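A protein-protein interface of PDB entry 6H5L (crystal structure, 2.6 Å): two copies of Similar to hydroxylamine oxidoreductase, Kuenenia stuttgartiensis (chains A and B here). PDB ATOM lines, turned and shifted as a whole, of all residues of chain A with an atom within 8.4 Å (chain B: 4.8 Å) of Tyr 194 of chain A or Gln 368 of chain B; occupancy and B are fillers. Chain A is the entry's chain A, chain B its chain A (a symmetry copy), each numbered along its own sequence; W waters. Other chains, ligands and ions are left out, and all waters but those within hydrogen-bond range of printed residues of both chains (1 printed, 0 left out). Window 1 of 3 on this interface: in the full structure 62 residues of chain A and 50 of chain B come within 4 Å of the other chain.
N of Met 49 of chain A lies within hydrogen-bond range of OH of Tyr 194 of chain A, 3.2 Å away. The backbone NH (N) of Tyr 192 of chain A lies within hydrogen-bond range of the backbone carbonyl oxygen (O) of Ala 187 of chain A (2.8 Å). O of Phe 369 of chain B is in hydrogen-bond range of NE2 of Gln 372 of chain B (2.9 Å).
Met 49 of chain A touches Lys 364 of chain B. CE of Met 49 of chain A touches OG of Ser 365 of chain B (3.3 Å). Leu 50 of chain A touches Ser 365 of chain B. Tyr 192 of chain A touches Gln 372 of chain B. Tyr 194 of chain A touches Ser 365 of chain B. Gln 368 of chain B touches Tyr 194 of chain A (CB to CG, 3.4 Å). O of Tyr 194 of chain A touches CD1 of Phe 369 of chain B, at 3.4 Å. Gly 195 of chain A touches Phe 369 of chain B (CA to CD1, 3.8 Å). Gln 372 of chain B touches Gly 195 of chain A (NE2 to CA, 3.4 Å). CB of Ser 365 of chain B touches ND1 of His 197 of chain A, 3.8 Å away.
Of chain A, only Tyr 194 (3.4 Å) comes within 4 Å of Gln 368 of chain B. Of the printed residues of chain B, Gly 191 of chain A touches Gln 372 (3.5 Å). Of the printed residues of chain B, Gly 195 of chain A touches Phe 369 and Gln 372. Of the printed residues of chain B, Tyr 192 of chain A touches Gln 372 (3.6 Å). Printed residues of chain B within 4 Å of Met 49 of chain A: Lys 364 and Ser 365. Lys 46 of chain A touches none of the printed residues of chain B.
Of the 20 printed residues of chain A, 7 touch a printed residue of chain B. Printed residues of chain A that touch a printed residue of chain B: Met 49, Leu 50, Gly 191, Tyr 192, Tyr 194, Gly 195 and His 197. Hydrophobic or aromatic side chains of chain B that line the printed part of chain A: Phe 369. Among the printed residues, 11 pairs touch across the chains.
No position is printed for both chains. Of the 11 pairs that touch across the chains among the printed residues, none has its exchanged pair printed and touching as well.
Water W1 lies within hydrogen-bond range of OG of Ser 365 of chain B (2.6 Å), N of Leu 50 of chain A (2.9 Å) and N of Met 49 of chain A (3.2 Å).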
ATOM      1  N   LEU A  34     -15.338 -23.010 -11.591  1.00  0.00           N
ATOM      2  CA  LEU A  34     -15.233 -22.129 -10.438  1.00  0.00           C
ATOM      3  C   LEU A  34     -16.421 -22.295  -9.504  1.00  0.00           C
ATOM      4  O   LEU A  34     -16.583 -21.507  -8.567  1.00  0.00           O
ATOM      5  CB  LEU A  34     -15.114 -20.670 -10.887  1.00  0.00           C
ATOM      6  CG  LEU A  34     -13.801 -20.258 -11.553  1.00  0.00           C
ATOM      7  CD1 LEU A  34     -13.857 -18.796 -11.958  1.00  0.00           C
ATOM      8  CD2 LEU A  34     -12.631 -20.514 -10.618  1.00  0.00           C
ATOM      9  N   LYS A  46     -15.930 -21.433  -2.596  1.00  0.00           N
ATOM     10  CA  LYS A  46     -15.747 -21.463  -4.038  1.00  0.00           C
ATOM     11  C   LYS A  46     -14.354 -20.954  -4.375  1.00  0.00           C
ATOM     12  O   LYS A  46     -13.777 -20.145  -3.644  1.00  0.00           O
ATOM     13  CB  LYS A  46     -16.806 -20.620  -4.762  1.00  0.00           C
ATOM     14  CG  LYS A  46     -18.223 -21.140  -4.594  1.00  0.00           C
ATOM     15  CD  LYS A  46     -19.177 -20.481  -5.574  1.00  0.00           C
ATOM     16  CE  LYS A  46     -20.574 -21.067  -5.456  1.00  0.00           C
ATOM     17  NZ  LYS A  46     -21.465 -20.604  -6.556  1.00  0.00           N
ATOM     18  N   ALA A  47     -13.814 -21.444  -5.485  1.00  0.00           N
ATOM     19  CA  ALA A  47     -12.457 -21.093  -5.873  1.00  0.00           C
ATOM     20  C   ALA A  47     -12.379 -19.649  -6.349  1.00  0.00           C
ATOM     21  O   ALA A  47     -13.337 -19.097  -6.898  1.00  0.00           O
ATOM     22  CB  ALA A  47     -11.961 -22.028  -6.973  1.00  0.00           C
ATOM     23  N   GLN A  48     -11.221 -19.033  -6.127  1.00  0.00           N
ATOM     24  CA  GLN A  48     -10.963 -17.717  -6.690  1.00  0.00           C
ATOM     25  C   GLN A  48     -10.822 -17.825  -8.206  1.00  0.00           C
ATOM     26  O   GLN A  48     -10.523 -18.892  -8.751  1.00  0.00           O
ATOM     27  CB  GLN A  48      -9.705 -17.104  -6.071  1.00  0.00           C
ATOM     28  CG  GLN A  48      -9.805 -16.890  -4.568  1.00  0.00           C
ATOM     29  CD  GLN A  48      -8.519 -16.361  -3.961  1.00  0.00           C
ATOM     30  OE1 GLN A  48      -8.045 -15.283  -4.319  1.00  0.00           O
ATOM     31  NE2 GLN A  48      -7.946 -17.122  -3.034  1.00  0.00           N
ATOM     32  N   MET A  49     -11.051 -16.699  -8.886  1.00  0.00           N
ATOM     33  CA  MET A  49     -11.081 -16.694 -10.347  1.00  0.00           C
ATOM     34  C   MET A  49      -9.786 -17.242 -10.940  1.00  0.00           C
ATOM     35  O   MET A  49      -9.811 -18.063 -11.865  1.00  0.00           O
ATOM     36  CB  MET A  49     -11.342 -15.277 -10.857  1.00  0.00           C
ATOM     37  CG  MET A  49     -12.741 -14.756 -10.583  1.00  0.00           C
ATOM     38  SD  MET A  49     -12.885 -12.998 -10.956  1.00  0.00           S
ATOM     39  CE  MET A  49     -11.888 -12.290  -9.647  1.00  0.00           C
ATOM     40  N   LEU A  50      -8.642 -16.809 -10.409  1.00  0.00           N
ATOM     41  CA  LEU A  50      -7.353 -17.179 -10.979  1.00  0.00           C
ATOM     42  C   LEU A  50      -6.990 -18.641 -10.753  1.00  0.00           C
ATOM     43  O   LEU A  50      -5.959 -19.088 -11.269  1.00  0.00           O
ATOM     44  CB  LEU A  50      -6.258 -16.283 -10.408  1.00  0.00           C
ATOM     45  CG  LEU A  50      -6.306 -14.821 -10.846  1.00  0.00           C
ATOM     46  CD1 LEU A  50      -5.654 -13.940  -9.800  1.00  0.00           C
ATOM     47  CD2 LEU A  50      -5.623 -14.653 -12.194  1.00  0.00           C
ATOM     48  N   ASP A  51      -7.797 -19.392 -10.001  1.00  0.00           N
ATOM     49  CA  ASP A  51      -7.541 -20.817  -9.842  1.00  0.00           C
ATOM     50  C   ASP A  51      -7.702 -21.578 -11.151  1.00  0.00           C
ATOM     51  O   ASP A  51      -7.219 -22.711 -11.256  1.00  0.00           O
ATOM     52  CB  ASP A  51      -8.459 -21.400  -8.768  1.00  0.00           C
ATOM     53  CG  ASP A  51      -8.130 -20.881  -7.381  1.00  0.00           C
ATOM     54  OD1 ASP A  51      -7.103 -20.184  -7.234  1.00  0.00           O
ATOM     55  OD2 ASP A  51      -8.893 -21.166  -6.436  1.00  0.00           O
ATOM     56  N   TYR A 184      -8.953 -21.655   5.651  1.00  0.00           N
ATOM     57  CA  TYR A 184      -9.119 -21.136   4.297  1.00  0.00           C
ATOM     58  C   TYR A 184     -10.598 -20.992   3.958  1.00  0.00           C
ATOM     59  O   TYR A 184     -11.049 -19.918   3.542  1.00  0.00           O
ATOM     60  CB  TYR A 184      -8.416 -22.054   3.291  1.00  0.00           C
ATOM     61  CG  TYR A 184      -8.337 -21.506   1.876  1.00  0.00           C
ATOM     62  CD1 TYR A 184      -9.436 -21.556   1.023  1.00  0.00           C
ATOM     63  CD2 TYR A 184      -7.158 -20.957   1.385  1.00  0.00           C
ATOM     64  CE1 TYR A 184      -9.368 -21.062  -0.265  1.00  0.00           C
ATOM     65  CE2 TYR A 184      -7.080 -20.461   0.094  1.00  0.00           C
ATOM     66  CZ  TYR A 184      -8.190 -20.518  -0.726  1.00  0.00           C
ATOM     67  OH  TYR A 184      -8.128 -20.030  -2.010  1.00  0.00           O
ATOM     68  N   ALA A 187     -12.373 -18.297   6.162  1.00  0.00           N
ATOM     69  CA  ALA A 187     -12.175 -16.935   5.674  1.00  0.00           C
ATOM     70  C   ALA A 187     -13.084 -16.636   4.487  1.00  0.00           C
ATOM     71  O   ALA A 187     -13.610 -15.522   4.365  1.00  0.00           O
ATOM     72  CB  ALA A 187     -10.708 -16.715   5.305  1.00  0.00           C
ATOM     73  N   ALA A 188     -13.286 -17.620   3.605  1.00  0.00           N
ATOM     74  CA  ALA A 188     -14.203 -17.438   2.485  1.00  0.00           C
ATOM     75  C   ALA A 188     -15.652 -17.359   2.948  1.00  0.00           C
ATOM     76  O   ALA A 188     -16.453 -16.632   2.349  1.00  0.00           O
ATOM     77  CB  ALA A 188     -14.030 -18.578   1.486  1.00  0.00           C
ATOM     78  N   GLY A 191     -16.392 -13.757   3.901  1.00  0.00           N
ATOM     79  CA  GLY A 191     -16.222 -12.748   2.879  1.00  0.00           C
ATOM     80  C   GLY A 191     -14.798 -12.322   2.605  1.00  0.00           C
ATOM     81  O   GLY A 191     -14.595 -11.291   1.953  1.00  0.00           O
ATOM     82  N   TYR A 192     -13.804 -13.079   3.073  1.00  0.00           N
ATOM     83  CA  TYR A 192     -12.399 -12.758   2.852  1.00  0.00           C
ATOM     84  C   TYR A 192     -11.714 -13.795   1.968  1.00  0.00           C
ATOM     85  O   TYR A 192     -10.529 -14.082   2.144  1.00  0.00           O
ATOM     86  CB  TYR A 192     -11.653 -12.628   4.180  1.00  0.00           C
ATOM     87  CG  TYR A 192     -12.385 -11.827   5.231  1.00  0.00           C
ATOM     88  CD1 TYR A 192     -12.614 -10.467   5.064  1.00  0.00           C
ATOM     89  CD2 TYR A 192     -12.832 -12.429   6.399  1.00  0.00           C
ATOM     90  CE1 TYR A 192     -13.282  -9.733   6.027  1.00  0.00           C
ATOM     91  CE2 TYR A 192     -13.498 -11.704   7.367  1.00  0.00           C
ATOM     92  CZ  TYR A 192     -13.720 -10.356   7.176  1.00  0.00           C
ATOM     93  OH  TYR A 192     -14.383  -9.630   8.138  1.00  0.00           O
ATOM     94  N   LEU A 193     -12.454 -14.372   1.018  1.00  0.00           N
ATOM     95  CA  LEU A 193     -11.867 -15.365   0.122  1.00  0.00           C
ATOM     96  C   LEU A 193     -10.718 -14.771  -0.682  1.00  0.00           C
ATOM     97  O   LEU A 193      -9.642 -15.370  -0.784  1.00  0.00           O
ATOM     98  CB  LEU A 193     -12.938 -15.925  -0.815  1.00  0.00           C
ATOM     99  CG  LEU A 193     -12.413 -16.784  -1.969  1.00  0.00           C
ATOM    100  CD1 LEU A 193     -11.872 -18.115  -1.464  1.00  0.00           C
ATOM    101  CD2 LEU A 193     -13.487 -16.994  -3.028  1.00  0.00           C
ATOM    102  N   TYR A 194     -10.930 -13.591  -1.262  1.00  0.00           N
ATOM    103  CA  TYR A 194      -9.910 -12.966  -2.093  1.00  0.00           C
ATOM    104  C   TYR A 194      -8.838 -12.248  -1.289  1.00  0.00           C
ATOM    105  O   TYR A 194      -7.868 -11.761  -1.880  1.00  0.00           O
ATOM    106  CB  TYR A 194     -10.564 -12.005  -3.085  1.00  0.00           C
ATOM    107  CG  TYR A 194     -11.226 -12.726  -4.234  1.00  0.00           C
ATOM    108  CD1 TYR A 194     -10.507 -13.052  -5.377  1.00  0.00           C
ATOM    109  CD2 TYR A 194     -12.561 -13.101  -4.168  1.00  0.00           C
ATOM    110  CE1 TYR A 194     -11.104 -13.722  -6.428  1.00  0.00           C
ATOM    111  CE2 TYR A 194     -13.166 -13.769  -5.214  1.00  0.00           C
ATOM    112  CZ  TYR A 194     -12.433 -14.077  -6.340  1.00  0.00           C
ATOM    113  OH  TYR A 194     -13.037 -14.743  -7.381  1.00  0.00           O
ATOM    114  N   GLY A 195      -8.981 -12.166   0.035  1.00  0.00           N
ATOM    115  CA  GLY A 195      -7.859 -11.765   0.862  1.00  0.00           C
ATOM    116  C   GLY A 195      -6.725 -12.765   0.836  1.00  0.00           C
ATOM    117  O   GLY A 195      -5.586 -12.415   1.163  1.00  0.00           O
ATOM    118  N   GLN A 196      -7.012 -14.005   0.438  1.00  0.00           N
ATOM    119  CA  GLN A 196      -6.011 -15.046   0.252  1.00  0.00           C
ATOM    120  C   GLN A 196      -5.497 -15.097  -1.183  1.00  0.00           C
ATOM    121  O   GLN A 196      -5.121 -16.172  -1.670  1.00  0.00           O
ATOM    122  CB  GLN A 196      -6.594 -16.394   0.676  1.00  0.00           C
ATOM    123  CG  GLN A 196      -7.194 -16.360   2.077  1.00  0.00           C
ATOM    124  CD  GLN A 196      -7.933 -17.630   2.438  1.00  0.00           C
ATOM    125  OE1 GLN A 196      -7.724 -18.196   3.511  1.00  0.00           O
ATOM    126  NE2 GLN A 196      -8.809 -18.080   1.549  1.00  0.00           N
ATOM    127  N   HIS A 197      -5.492 -13.949  -1.869  1.00  0.00           N
ATOM    128  CA  HIS A 197      -5.041 -13.878  -3.258  1.00  0.00           C
ATOM    129  C   HIS A 197      -3.616 -14.394  -3.407  1.00  0.00           C
ATOM    130  O   HIS A 197      -3.322 -15.197  -4.300  1.00  0.00           O
ATOM    131  CB  HIS A 197      -5.148 -12.433  -3.753  1.00  0.00           C
ATOM    132  CG  HIS A 197      -4.474 -12.180  -5.066  1.00  0.00           C
ATOM    133  ND1 HIS A 197      -5.138 -12.263  -6.272  1.00  0.00           N
ATOM    134  CD2 HIS A 197      -3.200 -11.828  -5.362  1.00  0.00           C
ATOM    135  CE1 HIS A 197      -4.301 -11.981  -7.253  1.00  0.00           C
ATOM    136  NE2 HIS A 197      -3.118 -11.714  -6.729  1.00  0.00           N
ATOM    137  N   GLY A 198      -2.710 -13.930  -2.544  1.00  0.00           N
ATOM    138  CA  GLY A 198      -1.334 -14.385  -2.604  1.00  0.00           C
ATOM    139  C   GLY A 198      -1.158 -15.848  -2.262  1.00  0.00           C
ATOM    140  O   GLY A 198      -0.177 -16.461  -2.694  1.00  0.00           O
ATOM    141  N   CYS A 199      -2.094 -16.425  -1.505  1.00  0.00           N
ATOM    142  CA  CYS A 199      -1.972 -17.825  -1.111  1.00  0.00           C
ATOM    143  C   CYS A 199      -2.116 -18.748  -2.317  1.00  0.00           C
ATOM    144  O   CYS A 199      -1.267 -19.618  -2.551  1.00  0.00           O
ATOM    145  CB  CYS A 199      -3.013 -18.161  -0.042  1.00  0.00           C
ATOM    146  SG  CYS A 199      -2.970 -17.084   1.412  1.00  0.00           S
ATOM    147  N   ASP A 200      -3.187 -18.574  -3.096  1.00  0.00           N
ATOM    148  CA  ASP A 200      -3.375 -19.393  -4.291  1.00  0.00           C
ATOM    149  C   ASP A 200      -2.276 -19.151  -5.316  1.00  0.00           C
ATOM    150  O   ASP A 200      -1.931 -20.058  -6.082  1.00  0.00           O
ATOM    151  CB  ASP A 200      -4.742 -19.111  -4.914  1.00  0.00           C
ATOM    152  CG  ASP A 200      -5.887 -19.397  -3.966  1.00  0.00           C
ATOM    153  OD1 ASP A 200      -5.638 -19.498  -2.745  1.00  0.00           O
ATOM    154  OD2 ASP A 200      -7.036 -19.530  -4.438  1.00  0.00           O
ATOM    155  N   TYR B 335     -16.901   0.925 -10.824  1.00  0.00           N
ATOM    156  CA  TYR B 335     -17.582   0.518 -12.046  1.00  0.00           C
ATOM    157  C   TYR B 335     -18.240   1.696 -12.763  1.00  0.00           C
ATOM    158  O   TYR B 335     -19.248   1.526 -13.451  1.00  0.00           O
ATOM    159  CB  TYR B 335     -18.603  -0.573 -11.740  1.00  0.00           C
ATOM    160  CG  TYR B 335     -17.973  -1.797 -11.118  1.00  0.00           C
ATOM    161  CD1 TYR B 335     -17.155  -2.633 -11.868  1.00  0.00           C
ATOM    162  CD2 TYR B 335     -18.179  -2.109  -9.782  1.00  0.00           C
ATOM    163  CE1 TYR B 335     -16.568  -3.749 -11.307  1.00  0.00           C
ATOM    164  CE2 TYR B 335     -17.595  -3.225  -9.211  1.00  0.00           C
ATOM    165  CZ  TYR B 335     -16.790  -4.042  -9.978  1.00  0.00           C
ATOM    166  OH  TYR B 335     -16.206  -5.154  -9.418  1.00  0.00           O
ATOM    167  N   LYS B 364      -9.492  -8.200 -12.000  1.00  0.00           N
ATOM    168  CA  LYS B 364     -10.739  -8.395 -11.265  1.00  0.00           C
ATOM    169  C   LYS B 364     -10.484  -8.979  -9.881  1.00  0.00           C
ATOM    170  O   LYS B 364     -11.245  -8.709  -8.945  1.00  0.00           O
ATOM    171  CB  LYS B 364     -11.690  -9.289 -12.063  1.00  0.00           C
ATOM    172  CG  LYS B 364     -12.551  -8.521 -13.054  1.00  0.00           C
ATOM    173  CD  LYS B 364     -12.925  -9.370 -14.256  1.00  0.00           C
ATOM    174  CE  LYS B 364     -13.719 -10.604 -13.868  1.00  0.00           C
ATOM    175  NZ  LYS B 364     -14.024 -11.443 -15.062  1.00  0.00           N
ATOM    176  N   SER B 365      -9.423  -9.772  -9.729  1.00  0.00           N
ATOM    177  CA  SER B 365      -9.044 -10.252  -8.403  1.00  0.00           C
ATOM    178  C   SER B 365      -8.452  -9.131  -7.559  1.00  0.00           C
ATOM    179  O   SER B 365      -8.625  -9.119  -6.334  1.00  0.00           O
ATOM    180  CB  SER B 365      -8.056 -11.408  -8.519  1.00  0.00           C
ATOM    181  OG  SER B 365      -8.611 -12.487  -9.251  1.00  0.00           O
ATOM    182  N   LEU B 366      -7.745  -8.190  -8.189  1.00  0.00           N
ATOM    183  CA  LEU B 366      -7.298  -6.998  -7.476  1.00  0.00           C
ATOM    184  C   LEU B 366      -8.481  -6.219  -6.919  1.00  0.00           C
ATOM    185  O   LEU B 366      -8.440  -5.741  -5.779  1.00  0.00           O
ATOM    186  CB  LEU B 366      -6.465  -6.110  -8.402  1.00  0.00           C
ATOM    187  CG  LEU B 366      -6.187  -4.685  -7.915  1.00  0.00           C
ATOM    188  CD1 LEU B 366      -5.304  -4.695  -6.675  1.00  0.00           C
ATOM    189  CD2 LEU B 366      -5.562  -3.841  -9.021  1.00  0.00           C
ATOM    190  N   ASP B 367      -9.545  -6.078  -7.714  1.00  0.00           N
ATOM    191  CA  ASP B 367     -10.745  -5.403  -7.232  1.00  0.00           C
ATOM    192  C   ASP B 367     -11.374  -6.158  -6.067  1.00  0.00           C
ATOM    193  O   ASP B 367     -11.795  -5.549  -5.076  1.00  0.00           O
ATOM    194  CB  ASP B 367     -11.752  -5.246  -8.373  1.00  0.00           C
ATOM    195  CG  ASP B 367     -11.208  -4.421  -9.525  1.00  0.00           C
ATOM    196  OD1 ASP B 367     -10.359  -3.539  -9.279  1.00  0.00           O
ATOM    197  OD2 ASP B 367     -11.633  -4.656 -10.677  1.00  0.00           O
ATOM    198  N   GLN B 368     -11.439  -7.488  -6.166  1.00  0.00           N
ATOM    199  CA  GLN B 368     -12.036  -8.282  -5.097  1.00  0.00           C
ATOM    200  C   GLN B 368     -11.219  -8.192  -3.817  1.00  0.00           C
ATOM    201  O   GLN B 368     -11.784  -8.120  -2.719  1.00  0.00           O
ATOM    202  CB  GLN B 368     -12.182  -9.736  -5.539  1.00  0.00           C
ATOM    203  CG  GLN B 368     -13.229  -9.944  -6.616  1.00  0.00           C
ATOM    204  CD  GLN B 368     -14.593  -9.422  -6.207  1.00  0.00           C
ATOM    205  OE1 GLN B 368     -15.282  -8.769  -6.991  1.00  0.00           O
ATOM    206  NE2 GLN B 368     -14.992  -9.710  -4.972  1.00  0.00           N
ATOM    207  N   PHE B 369      -9.890  -8.198  -3.933  1.00  0.00           N
ATOM    208  CA  PHE B 369      -9.049  -8.031  -2.751  1.00  0.00           C
ATOM    209  C   PHE B 369      -9.298  -6.682  -2.089  1.00  0.00           C
ATOM    210  O   PHE B 369      -9.342  -6.586  -0.858  1.00  0.00           O
ATOM    211  CB  PHE B 369      -7.573  -8.181  -3.123  1.00  0.00           C
ATOM    212  CG  PHE B 369      -6.629  -7.884  -1.992  1.00  0.00           C
ATOM    213  CD1 PHE B 369      -6.261  -8.878  -1.097  1.00  0.00           C
ATOM    214  CD2 PHE B 369      -6.110  -6.610  -1.819  1.00  0.00           C
ATOM    215  CE1 PHE B 369      -5.394  -8.607  -0.054  1.00  0.00           C
ATOM    216  CE2 PHE B 369      -5.247  -6.333  -0.777  1.00  0.00           C
ATOM    217  CZ  PHE B 369      -4.887  -7.332   0.105  1.00  0.00           C
ATOM    218  N   MET B 370      -9.462  -5.630  -2.892  1.00  0.00           N
ATOM    219  CA  MET B 370      -9.669  -4.299  -2.330  1.00  0.00           C
ATOM    220  C   MET B 370     -11.050  -4.168  -1.701  1.00  0.00           C
ATOM    221  O   MET B 370     -11.212  -3.478  -0.685  1.00  0.00           O
ATOM    222  CB  MET B 370      -9.459  -3.242  -3.410  1.00  0.00           C
ATOM    223  CG  MET B 370      -8.019  -3.129  -3.857  1.00  0.00           C
ATOM    224  SD  MET B 370      -6.943  -2.805  -2.452  1.00  0.00           S
ATOM    225  CE  MET B 370      -7.251  -1.061  -2.186  1.00  0.00           C
ATOM    226  N   PHE B 371     -12.058  -4.814  -2.287  1.00  0.00           N
ATOM    227  CA  PHE B 371     -13.397  -4.773  -1.705  1.00  0.00           C
ATOM    228  C   PHE B 371     -13.417  -5.433  -0.332  1.00  0.00           C
ATOM    229  O   PHE B 371     -13.989  -4.894   0.622  1.00  0.00           O
ATOM    230  CB  PHE B 371     -14.399  -5.445  -2.647  1.00  0.00           C
ATOM    231  CG  PHE B 371     -14.750  -4.616  -3.851  1.00  0.00           C
ATOM    232  CD1 PHE B 371     -14.905  -3.244  -3.742  1.00  0.00           C
ATOM    233  CD2 PHE B 371     -14.917  -5.208  -5.091  1.00  0.00           C
ATOM    234  CE1 PHE B 371     -15.226  -2.479  -4.847  1.00  0.00           C
ATOM    235  CE2 PHE B 371     -15.237  -4.446  -6.201  1.00  0.00           C
ATOM    236  CZ  PHE B 371     -15.393  -3.080  -6.079  1.00  0.00           C
ATOM    237  N   GLN B 372     -12.787  -6.605  -0.210  1.00  0.00           N
ATOM    238  CA  GLN B 372     -12.768  -7.291   1.077  1.00  0.00           C
ATOM    239  C   GLN B 372     -11.817  -6.616   2.058  1.00  0.00           C
ATOM    240  O   GLN B 372     -12.047  -6.663   3.272  1.00  0.00           O
ATOM    241  CB  GLN B 372     -12.399  -8.765   0.883  1.00  0.00           C
ATOM    242  CG  GLN B 372     -10.991  -9.023   0.368  1.00  0.00           C
ATOM    243  CD  GLN B 372      -9.973  -9.136   1.487  1.00  0.00           C
ATOM    244  OE1 GLN B 372     -10.227  -9.771   2.511  1.00  0.00           O
ATOM    245  NE2 GLN B 372      -8.815  -8.512   1.300  1.00  0.00           N
HETATM  246  O   HOH W   1      -8.439 -14.911  -8.226  1.00  0.00           O
